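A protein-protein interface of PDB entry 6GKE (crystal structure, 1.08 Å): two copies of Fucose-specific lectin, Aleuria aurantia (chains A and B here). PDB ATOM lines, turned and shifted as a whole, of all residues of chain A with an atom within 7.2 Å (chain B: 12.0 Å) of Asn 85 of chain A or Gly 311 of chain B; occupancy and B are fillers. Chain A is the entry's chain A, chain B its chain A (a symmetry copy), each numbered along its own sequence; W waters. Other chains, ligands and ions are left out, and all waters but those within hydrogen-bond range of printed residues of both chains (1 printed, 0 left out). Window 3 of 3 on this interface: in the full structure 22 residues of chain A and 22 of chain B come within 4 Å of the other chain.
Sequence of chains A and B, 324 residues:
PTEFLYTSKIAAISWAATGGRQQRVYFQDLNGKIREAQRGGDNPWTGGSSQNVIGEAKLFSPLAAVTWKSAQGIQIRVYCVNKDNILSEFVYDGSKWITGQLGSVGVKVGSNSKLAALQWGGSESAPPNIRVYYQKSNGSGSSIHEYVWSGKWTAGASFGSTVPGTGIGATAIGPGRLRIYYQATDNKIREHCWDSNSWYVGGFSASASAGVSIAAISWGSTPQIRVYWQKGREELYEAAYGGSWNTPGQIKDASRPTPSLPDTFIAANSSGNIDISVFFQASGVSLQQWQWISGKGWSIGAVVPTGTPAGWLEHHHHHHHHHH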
ATOM      1  N   LYS A  58     -26.816  18.018  31.750  1.00  0.00           N
ATOM      2  CA  LYS A  58     -26.189  19.121  31.046  1.00  0.00           C
ATOM      3  C   LYS A  58     -25.713  20.147  32.074  1.00  0.00           C
ATOM      4  O   LYS A  58     -26.296  20.290  33.147  1.00  0.00           O
ATOM      5  CB  LYS A  58     -27.133  19.773  30.032  1.00  0.00           C
ATOM      6  CG  LYS A  58     -28.214  20.684  30.599  1.00  0.00           C
ATOM      7  CD  LYS A  58     -28.938  21.448  29.513  1.00  0.00           C
ATOM      8  CE  LYS A  58     -29.934  22.451  30.049  1.00  0.00           C
ATOM      9  NZ  LYS A  58     -30.509  23.248  28.940  1.00  0.00           N
ATOM     10  N   LEU A  59     -24.647  20.871  31.742  1.00  0.00           N
ATOM     11  CA  LEU A  59     -24.202  21.934  32.627  1.00  0.00           C
ATOM     12  C   LEU A  59     -25.352  22.935  32.797  1.00  0.00           C
ATOM     13  O   LEU A  59     -26.017  23.293  31.830  1.00  0.00           O
ATOM     14  CB  LEU A  59     -22.936  22.607  32.088  1.00  0.00           C
ATOM     15  CG  LEU A  59     -21.610  21.953  32.485  1.00  0.00           C
ATOM     16  CD1 LEU A  59     -21.344  22.087  33.976  1.00  0.00           C
ATOM     17  CD2 LEU A  59     -21.523  20.498  32.071  1.00  0.00           C
ATOM     18  N   PRO A  62     -31.593  22.254  35.143  1.00  0.00           N
ATOM     19  CA  PRO A  62     -32.517  22.366  36.265  1.00  0.00           C
ATOM     20  C   PRO A  62     -32.525  21.047  37.052  1.00  0.00           C
ATOM     21  O   PRO A  62     -32.106  20.001  36.536  1.00  0.00           O
ATOM     22  CB  PRO A  62     -33.851  22.663  35.578  1.00  0.00           C
ATOM     23  CG  PRO A  62     -33.733  21.938  34.258  1.00  0.00           C
ATOM     24  CD  PRO A  62     -32.290  22.145  33.848  1.00  0.00           C
ATOM     25  N   CYS A  80     -33.727  15.996  36.115  1.00  0.00           N
ATOM     26  CA  CYS A  80     -32.747  16.856  35.488  1.00  0.00           C
ATOM     27  C   CYS A  80     -32.968  16.793  33.977  1.00  0.00           C
ATOM     28  O   CYS A  80     -33.934  16.189  33.518  1.00  0.00           O
ATOM     29  CB  CYS A  80     -31.340  16.427  35.882  1.00  0.00           C
ATOM     30  SG  CYS A  80     -30.906  14.770  35.288  1.00  0.00           S
ATOM     31  N   VAL A  81     -32.077  17.417  33.209  1.00  0.00           N
ATOM     32  CA  VAL A  81     -32.129  17.457  31.775  1.00  0.00           C
ATOM     33  C   VAL A  81     -30.765  16.985  31.223  1.00  0.00           C
ATOM     34  O   VAL A  81     -29.741  17.454  31.726  1.00  0.00           O
ATOM     35  CB  VAL A  81     -32.502  18.902  31.383  1.00  0.00           C
ATOM     36  CG1 VAL A  81     -32.537  19.090  29.883  1.00  0.00           C
ATOM     37  CG2 VAL A  81     -33.835  19.327  31.993  1.00  0.00           C
ATOM     38  N   ASN A  82     -30.750  16.154  30.178  1.00  0.00           N
ATOM     39  CA  ASN A  82     -29.495  15.736  29.568  1.00  0.00           C
ATOM     40  C   ASN A  82     -29.052  16.774  28.525  1.00  0.00           C
ATOM     41  O   ASN A  82     -29.661  17.826  28.360  1.00  0.00           O
ATOM     42  CB  ASN A  82     -29.593  14.300  29.050  1.00  0.00           C
ATOM     43  CG  ASN A  82     -30.400  14.144  27.780  1.00  0.00           C
ATOM     44  OD1 ASN A  82     -30.819  15.122  27.163  1.00  0.00           O
ATOM     45  ND2 ASN A  82     -30.624  12.901  27.380  1.00  0.00           N
ATOM     46  N   LYS A  83     -27.973  16.473  27.800  1.00  0.00           N
ATOM     47  CA  LYS A  83     -27.362  17.440  26.890  1.00  0.00           C
ATOM     48  C   LYS A  83     -28.203  17.646  25.633  1.00  0.00           C
ATOM     49  O   LYS A  83     -27.947  18.577  24.884  1.00  0.00           O
ATOM     50  CB  LYS A  83     -25.940  17.026  26.520  1.00  0.00           C
ATOM     51  CG  LYS A  83     -24.949  17.387  27.609  1.00  0.00           C
ATOM     52  CD  LYS A  83     -23.569  16.883  27.353  1.00  0.00           C
ATOM     53  CE  LYS A  83     -22.631  17.204  28.493  1.00  0.00           C
ATOM     54  NZ  LYS A  83     -21.290  16.635  28.237  1.00  0.00           N
ATOM     55  N   ASP A  84     -29.207  16.784  25.426  1.00  0.00           N
ATOM     56  CA  ASP A  84     -30.175  16.937  24.334  1.00  0.00           C
ATOM     57  C   ASP A  84     -31.488  17.547  24.846  1.00  0.00           C
ATOM     58  O   ASP A  84     -32.493  17.539  24.138  1.00  0.00           O
ATOM     59  CB  ASP A  84     -30.403  15.597  23.635  1.00  0.00           C
ATOM     60  CG  ASP A  84     -29.162  15.102  22.910  1.00  0.00           C
ATOM     61  OD1 ASP A  84     -28.550  15.909  22.191  1.00  0.00           O
ATOM     62  OD2 ASP A  84     -28.803  13.928  23.096  1.00  0.00           O
ATOM     63  N   ASN A  85     -31.468  18.099  26.063  1.00  0.00           N
ATOM     64  CA  ASN A  85     -32.632  18.730  26.673  1.00  0.00           C
ATOM     65  C   ASN A  85     -33.793  17.738  26.815  1.00  0.00           C
ATOM     66  O   ASN A  85     -34.952  18.117  26.710  1.00  0.00           O
ATOM     67  CB  ASN A  85     -33.043  20.001  25.931  1.00  0.00           C
ATOM     68  CG  ASN A  85     -32.135  21.150  26.295  1.00  0.00           C
ATOM     69  OD1 ASN A  85     -31.950  21.434  27.479  1.00  0.00           O
ATOM     70  ND2 ASN A  85     -31.554  21.797  25.297  1.00  0.00           N
ATOM     71  N   ILE A  86     -33.471  16.477  27.112  1.00  0.00           N
ATOM     72  CA  ILE A  86     -34.486  15.476  27.400  1.00  0.00           C
ATOM     73  C   ILE A  86     -34.592  15.315  28.916  1.00  0.00           C
ATOM     74  O   ILE A  86     -33.593  15.134  29.608  1.00  0.00           O
ATOM     75  CB  ILE A  86     -34.170  14.140  26.700  1.00  0.00           C
ATOM     76  CG1 ILE A  86     -34.081  14.308  25.181  1.00  0.00           C
ATOM     77  CG2 ILE A  86     -35.180  13.074  27.087  1.00  0.00           C
ATOM     78  CD1 ILE A  86     -35.354  14.796  24.533  1.00  0.00           C
ATOM     79  N   LEU A  87     -35.828  15.385  29.413  1.00  0.00           N
ATOM     80  CA  LEU A  87     -36.137  15.211  30.823  1.00  0.00           C
ATOM     81  C   LEU A  87     -35.671  13.822  31.262  1.00  0.00           C
ATOM     82  O   LEU A  87     -36.029  12.824  30.647  1.00  0.00           O
ATOM     83  CB  LEU A  87     -37.646  15.389  31.003  1.00  0.00           C
ATOM     84  CG  LEU A  87     -38.166  15.325  32.434  1.00  0.00           C
ATOM     85  CD1 LEU A  87     -37.536  16.394  33.318  1.00  0.00           C
ATOM     86  CD2 LEU A  87     -39.677  15.452  32.420  1.00  0.00           C
ATOM     87  N   SER A  88     -34.879  13.787  32.338  1.00  0.00           N
ATOM     88  CA  SER A  88     -34.179  12.601  32.784  1.00  0.00           C
ATOM     89  C   SER A  88     -34.349  12.444  34.298  1.00  0.00           C
ATOM     90  O   SER A  88     -34.725  13.382  35.001  1.00  0.00           O
ATOM     91  CB  SER A  88     -32.719  12.681  32.391  1.00  0.00           C
ATOM     92  OG  SER A  88     -32.572  12.817  30.984  1.00  0.00           O
ATOM     93  N   GLY A 106     -38.836  10.530  26.219  1.00  0.00           N
ATOM     94  CA  GLY A 106     -38.574  11.521  25.167  1.00  0.00           C
ATOM     95  C   GLY A 106     -39.321  12.830  25.370  1.00  0.00           C
ATOM     96  O   GLY A 106     -39.848  13.416  24.414  1.00  0.00           O
ATOM     97  N   VAL A 107     -39.310  13.339  26.602  1.00  0.00           N
ATOM     98  CA  VAL A 107     -39.910  14.638  26.902  1.00  0.00           C
ATOM     99  C   VAL A 107     -38.857  15.727  26.685  1.00  0.00           C
ATOM    100  O   VAL A 107     -37.892  15.815  27.445  1.00  0.00           O
ATOM    101  CB  VAL A 107     -40.448  14.671  28.343  1.00  0.00           C
ATOM    102  CG1 VAL A 107     -41.061  16.029  28.664  1.00  0.00           C
ATOM    103  CG2 VAL A 107     -41.448  13.549  28.599  1.00  0.00           C
ATOM    104  N   LYS A 108     -39.036  16.546  25.646  1.00  0.00           N
ATOM    105  CA  LYS A 108     -38.111  17.642  25.369  1.00  0.00           C
ATOM    106  C   LYS A 108     -38.490  18.846  26.241  1.00  0.00           C
ATOM    107  O   LYS A 108     -39.655  19.228  26.342  1.00  0.00           O
ATOM    108  CB  LYS A 108     -38.116  17.986  23.876  1.00  0.00           C
ATOM    109  CG  LYS A 108     -37.050  18.979  23.427  1.00  0.00           C
ATOM    110  CD  LYS A 108     -35.678  18.367  23.237  1.00  0.00           C
ATOM    111  CE  LYS A 108     -34.757  19.215  22.388  1.00  0.00           C
ATOM    112  NZ  LYS A 108     -33.668  18.404  21.795  1.00  0.00           N
ATOM    113  N   VAL A 109     -37.471  19.438  26.854  1.00  0.00           N
ATOM    114  CA  VAL A 109     -37.615  20.548  27.770  1.00  0.00           C
ATOM    115  C   VAL A 109     -36.944  21.780  27.155  1.00  0.00           C
ATOM    116  O   VAL A 109     -35.898  21.678  26.514  1.00  0.00           O
ATOM    117  CB  VAL A 109     -37.001  20.158  29.126  1.00  0.00           C
ATOM    118  CG1 VAL A 109     -37.022  21.273  30.155  1.00  0.00           C
ATOM    119  CG2 VAL A 109     -37.674  18.923  29.694  1.00  0.00           C
ATOM    120  N   GLY A 110     -37.559  22.951  27.341  1.00  0.00           N
ATOM    121  CA  GLY A 110     -36.928  24.199  26.925  1.00  0.00           C
ATOM    122  C   GLY A 110     -35.575  24.368  27.601  1.00  0.00           C
ATOM    123  O   GLY A 110     -35.411  24.019  28.770  1.00  0.00           O
ATOM    124  N   SER A 111     -34.589  24.916  26.886  1.00  0.00           N
ATOM    125  CA  SER A 111     -33.227  24.927  27.418  1.00  0.00           C
ATOM    126  C   SER A 111     -33.146  25.673  28.756  1.00  0.00           C
ATOM    127  O   SER A 111     -32.336  25.293  29.603  1.00  0.00           O
ATOM    128  CB  SER A 111     -32.253  25.484  26.423  1.00  0.00           C
ATOM    129  OG  SER A 111     -32.567  26.829  26.132  1.00  0.00           O
ATOM    130  N   ASN A 112     -33.958  26.723  28.932  1.00  0.00           N
ATOM    131  CA  ASN A 112     -33.916  27.540  30.148  1.00  0.00           C
ATOM    132  C   ASN A 112     -35.024  27.162  31.141  1.00  0.00           C
ATOM    133  O   ASN A 112     -35.264  27.898  32.107  1.00  0.00           O
ATOM    134  CB  ASN A 112     -34.010  29.033  29.828  1.00  0.00           C
ATOM    135  CG  ASN A 112     -33.530  29.900  30.975  1.00  0.00           C
ATOM    136  OD1 ASN A 112     -32.561  29.566  31.662  1.00  0.00           O
ATOM    137  ND2 ASN A 112     -34.192  31.027  31.180  1.00  0.00           N
ATOM    138  N   SER A 113     -35.692  26.024  30.930  1.00  0.00           N
ATOM    139  CA  SER A 113     -36.757  25.606  31.833  1.00  0.00           C
ATOM    140  C   SER A 113     -36.204  25.323  33.227  1.00  0.00           C
ATOM    141  O   SER A 113     -35.115  24.766  33.372  1.00  0.00           O
ATOM    142  CB  SER A 113     -37.437  24.367  31.331  1.00  0.00           C
ATOM    143  OG  SER A 113     -38.560  24.025  32.131  1.00  0.00           O
ATOM    144  N   PRO B   1     -25.889  30.534  29.635  1.00  0.00           N
ATOM    145  CA  PRO B   1     -24.656  30.342  30.387  1.00  0.00           C
ATOM    146  C   PRO B   1     -23.465  30.188  29.436  1.00  0.00           C
ATOM    147  O   PRO B   1     -23.646  30.041  28.218  1.00  0.00           O
ATOM    148  CB  PRO B   1     -24.879  29.069  31.215  1.00  0.00           C
ATOM    149  CG  PRO B   1     -25.896  28.295  30.429  1.00  0.00           C
ATOM    150  CD  PRO B   1     -26.719  29.335  29.704  1.00  0.00           C
ATOM    151  N   THR B   2     -22.262  30.234  30.010  1.00  0.00           N
ATOM    152  CA  THR B   2     -21.033  30.085  29.250  1.00  0.00           C
ATOM    153  C   THR B   2     -20.138  29.059  29.944  1.00  0.00           C
ATOM    154  O   THR B   2     -20.492  28.515  30.991  1.00  0.00           O
ATOM    155  CB  THR B   2     -20.286  31.416  29.091  1.00  0.00           C
ATOM    156  OG1 THR B   2     -19.600  31.670  30.319  1.00  0.00           O
ATOM    157  CG2 THR B   2     -21.192  32.571  28.724  1.00  0.00           C
ATOM    158  N   GLU B   3     -18.956  28.851  29.357  1.00  0.00           N
ATOM    159  CA  GLU B   3     -17.989  27.921  29.927  1.00  0.00           C
ATOM    160  C   GLU B   3     -16.892  28.663  30.704  1.00  0.00           C
ATOM    161  O   GLU B   3     -15.917  28.055  31.110  1.00  0.00           O
ATOM    162  CB  GLU B   3     -17.470  27.016  28.814  1.00  0.00           C
ATOM    163  CG  GLU B   3     -18.590  26.202  28.195  1.00  0.00           C
ATOM    164  CD  GLU B   3     -18.192  25.351  27.006  1.00  0.00           C
ATOM    165  OE1 GLU B   3     -17.381  25.824  26.180  1.00  0.00           O
ATOM    166  OE2 GLU B   3     -18.693  24.214  26.918  1.00  0.00           O
ATOM    167  N   LEU B  30     -14.619  25.563  32.736  1.00  0.00           N
ATOM    168  CA  LEU B  30     -15.169  24.727  33.814  1.00  0.00           C
ATOM    169  C   LEU B  30     -14.361  23.441  34.009  1.00  0.00           C
ATOM    170  O   LEU B  30     -14.415  22.851  35.089  1.00  0.00           O
ATOM    171  CB  LEU B  30     -16.623  24.368  33.499  1.00  0.00           C
ATOM    172  CG  LEU B  30     -17.572  25.549  33.342  1.00  0.00           C
ATOM    173  CD1 LEU B  30     -18.955  25.055  32.963  1.00  0.00           C
ATOM    174  CD2 LEU B  30     -17.632  26.381  34.609  1.00  0.00           C
ATOM    175  N   GLY B 307     -17.506  30.483  25.171  1.00  0.00           N
ATOM    176  CA  GLY B 307     -18.091  29.171  24.967  1.00  0.00           C
ATOM    177  C   GLY B 307     -19.551  29.111  25.378  1.00  0.00           C
ATOM    178  O   GLY B 307     -20.066  29.976  26.084  1.00  0.00           O
ATOM    179  N   THR B 308     -20.224  28.058  24.911  1.00  0.00           N
ATOM    180  CA  THR B 308     -21.599  27.756  25.263  1.00  0.00           C
ATOM    181  C   THR B 308     -21.685  26.271  25.582  1.00  0.00           C
ATOM    182  O   THR B 308     -21.328  25.447  24.745  1.00  0.00           O
ATOM    183  CB  THR B 308     -22.572  28.090  24.126  1.00  0.00           C
ATOM    184  OG1 THR B 308     -22.432  29.466  23.778  1.00  0.00           O
ATOM    185  CG2 THR B 308     -24.016  27.831  24.492  1.00  0.00           C
ATOM    186  N   PRO B 309     -22.149  25.878  26.785  1.00  0.00           N
ATOM    187  CA  PRO B 309     -22.240  24.461  27.114  1.00  0.00           C
ATOM    188  C   PRO B 309     -23.280  23.746  26.242  1.00  0.00           C
ATOM    189  O   PRO B 309     -24.251  24.348  25.783  1.00  0.00           O
ATOM    190  CB  PRO B 309     -22.655  24.428  28.589  1.00  0.00           C
ATOM    191  CG  PRO B 309     -23.231  25.800  28.873  1.00  0.00           C
ATOM    192  CD  PRO B 309     -22.613  26.749  27.874  1.00  0.00           C
ATOM    193  N   ALA B 310     -23.068  22.445  26.049  1.00  0.00           N
ATOM    194  CA  ALA B 310     -24.021  21.605  25.354  1.00  0.00           C
ATOM    195  C   ALA B 310     -25.388  21.706  26.038  1.00  0.00           C
ATOM    196  O   ALA B 310     -25.487  21.753  27.264  1.00  0.00           O
ATOM    197  CB  ALA B 310     -23.532  20.179  25.318  1.00  0.00           C
ATOM    198  N   GLY B 311     -26.438  21.738  25.215  1.00  0.00           N
ATOM    199  CA  GLY B 311     -27.806  21.838  25.690  1.00  0.00           C
ATOM    200  C   GLY B 311     -28.294  23.275  25.796  1.00  0.00           C
ATOM    201  O   GLY B 311     -29.397  23.516  26.280  1.00  0.00           O
ATOM    202  N   TRP B 312     -27.473  24.223  25.336  1.00  0.00           N
ATOM    203  CA  TRP B 312     -27.817  25.633  25.329  1.00  0.00           C
ATOM    204  C   TRP B 312     -27.484  26.220  23.954  1.00  0.00           C
ATOM    205  O   TRP B 312     -26.586  25.721  23.293  1.00  0.00           O
ATOM    206  CB  TRP B 312     -27.053  26.363  26.433  1.00  0.00           C
ATOM    207  CG  TRP B 312     -27.373  25.897  27.817  1.00  0.00           C
ATOM    208  CD1 TRP B 312     -26.789  24.876  28.508  1.00  0.00           C
ATOM    209  CD2 TRP B 312     -28.371  26.454  28.688  1.00  0.00           C
ATOM    210  NE1 TRP B 312     -27.352  24.767  29.751  1.00  0.00           N
ATOM    211  CE2 TRP B 312     -28.317  25.727  29.895  1.00  0.00           C
ATOM    212  CE3 TRP B 312     -29.284  27.508  28.569  1.00  0.00           C
ATOM    213  CZ2 TRP B 312     -29.139  26.038  30.975  1.00  0.00           C
ATOM    214  CZ3 TRP B 312     -30.091  27.816  29.639  1.00  0.00           C
ATOM    215  CH2 TRP B 312     -30.003  27.100  30.830  1.00  0.00           C
HETATM  216  O   HOH W   1     -23.737  20.660  29.054  1.00  0.00           O
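Water W1 lies within hydrogen-bond range of O of Ala 310 of chain B and N of Leu 59 of chain A.
No position is printed for both chains.
The backbone carbonyl oxygen (O) of Val 81 of chain A lies within hydrogen-bond range of the backbone NH (N) of Lys 58 of chain A (3.0 Å). The side-chain amino group (NZ) of Lys 58 of chain A is in hydrogen-bond range of the side-chain amide oxygen (OD1) of Asn 85 of chain A, at 2.7 Å. The side-chain amino group (NZ) of Lys 58 of chain A is in hydrogen-bond range of the backbone carbonyl oxygen (O) of Ser 111 of chain A (2.8 Å). The side-chain amide oxygen of Asn 82 of chain A sits at hydrogen-bond distance from the backbone NH of Asn 85 of chain A (3.2 Å). O of Asn 85 of chain A is in hydrogen-bond range of N of Val 109 of chain A (2.8 Å). The backbone NH of Leu 30 of chain B is in hydrogen-bond range of the backbone carbonyl oxygen of Glu 3 of chain B, 3.2 Å away.
The side-chain amino group (NZ) of Lys 58 of chain A sits at hydrogen-bond distance from the backbone carbonyl oxygen (O) of Gly 311 of chain B (2.9 Å). The backbone carbonyl oxygen (O) of Leu 59 of chain A is in hydrogen-bond range of the indole nitrogen (NE1) of Trp 312 of chain B. The side-chain amide nitrogen (ND2) of Asn 85 of chain A lies within hydrogen-bond range of the backbone carbonyl oxygen (O) of Gly 311 of chain B.
Of the 10 printed residues of chain B, 5 touch a printed residue of chain A. Of the 20 printed residues of chain A, 6 touch a printed residue of chain B. Hydrophobic or aromatic side chains of chain A that line the printed part of chain B: Leu 59. Among the printed residues, 12 pairs touch across the chains.
Asn 85 of chain A touches just one residue of chain B: Gly 311. Of the printed residues of chain A, Gly 311 of chain B touches Lys 58 (2.9 Å), Lys 83 (3.4 Å), Asn 85 (2.9 Å) and Ser 111 (3.5 Å). Of the printed residues of chain B, Lys 58 of chain A touches Ala 310, Gly 311 and Trp 312. Asp 84 of chain A touches none of the printed residues of chain B. No residue of chain B comes within 4 Å of Ile 86 of chain A. No residue of chain B comes within 4 Å of Val 109 of chain A. No residue of chain B comes within 4 Å of Gly 110 of chain A. Ser 111 of chain A touches two residues of chain B. Of the printed residues of chain A, Leu 30 of chain B touches Leu 59. Of the printed residues of chain B, Lys 83 of chain A touches Ala 310 (3.9 Å) and Gly 311 (3.4 Å). Printed residues of chain A within 4 Å of Trp 312 of chain B: Lys 58, Leu 59, Ser 111 and Asn 112. Of the printed residues of chain A, Pro 309 of chain B touches Leu 59 (3.95 Å). Printed residues of chain B within 4 Å of Leu 59 of chain A: Leu 30, Pro 309 and Trp 312. Ser 88 of chain A touches none of the printed residues of chain B. Pro 62 of chain A touches none of the printed residues of chain B. The nearest residue of chain B that does not touch Asn 85 of chain A is Trp 312 of chain B (4.7 Å). The nearest printed residue of chain A that does not touch Leu 30 of chain B is Lys 58 of chain A (8.4 Å).
Ala 310 of chain B touches Lys 58 of chain A (O to CB, 3.8 Å). NZ of Lys 58 of chain A touches CE2 of Trp 312 of chain B, at 3.4 Å. Leu 30 of chain B touches Leu 59 of chain A (CD1 to CD1, 3.9 Å). Leu 59 of chain A touches Pro 309 of chain B. CB of Ala 310 of chain B touches CD of Lys 83 of chain A (3.9 Å). CA of Gly 311 of chain B touches O of Lys 83 of chain A, at 3.4 Å. Gly 311 of chain B touches Ser 111 of chain A. Trp 312 of chain B touches Ser 111 of chain A. CZ3 of Trp 312 of chain B touches OD1 of Asn 112 of chain A (3.6 Å).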
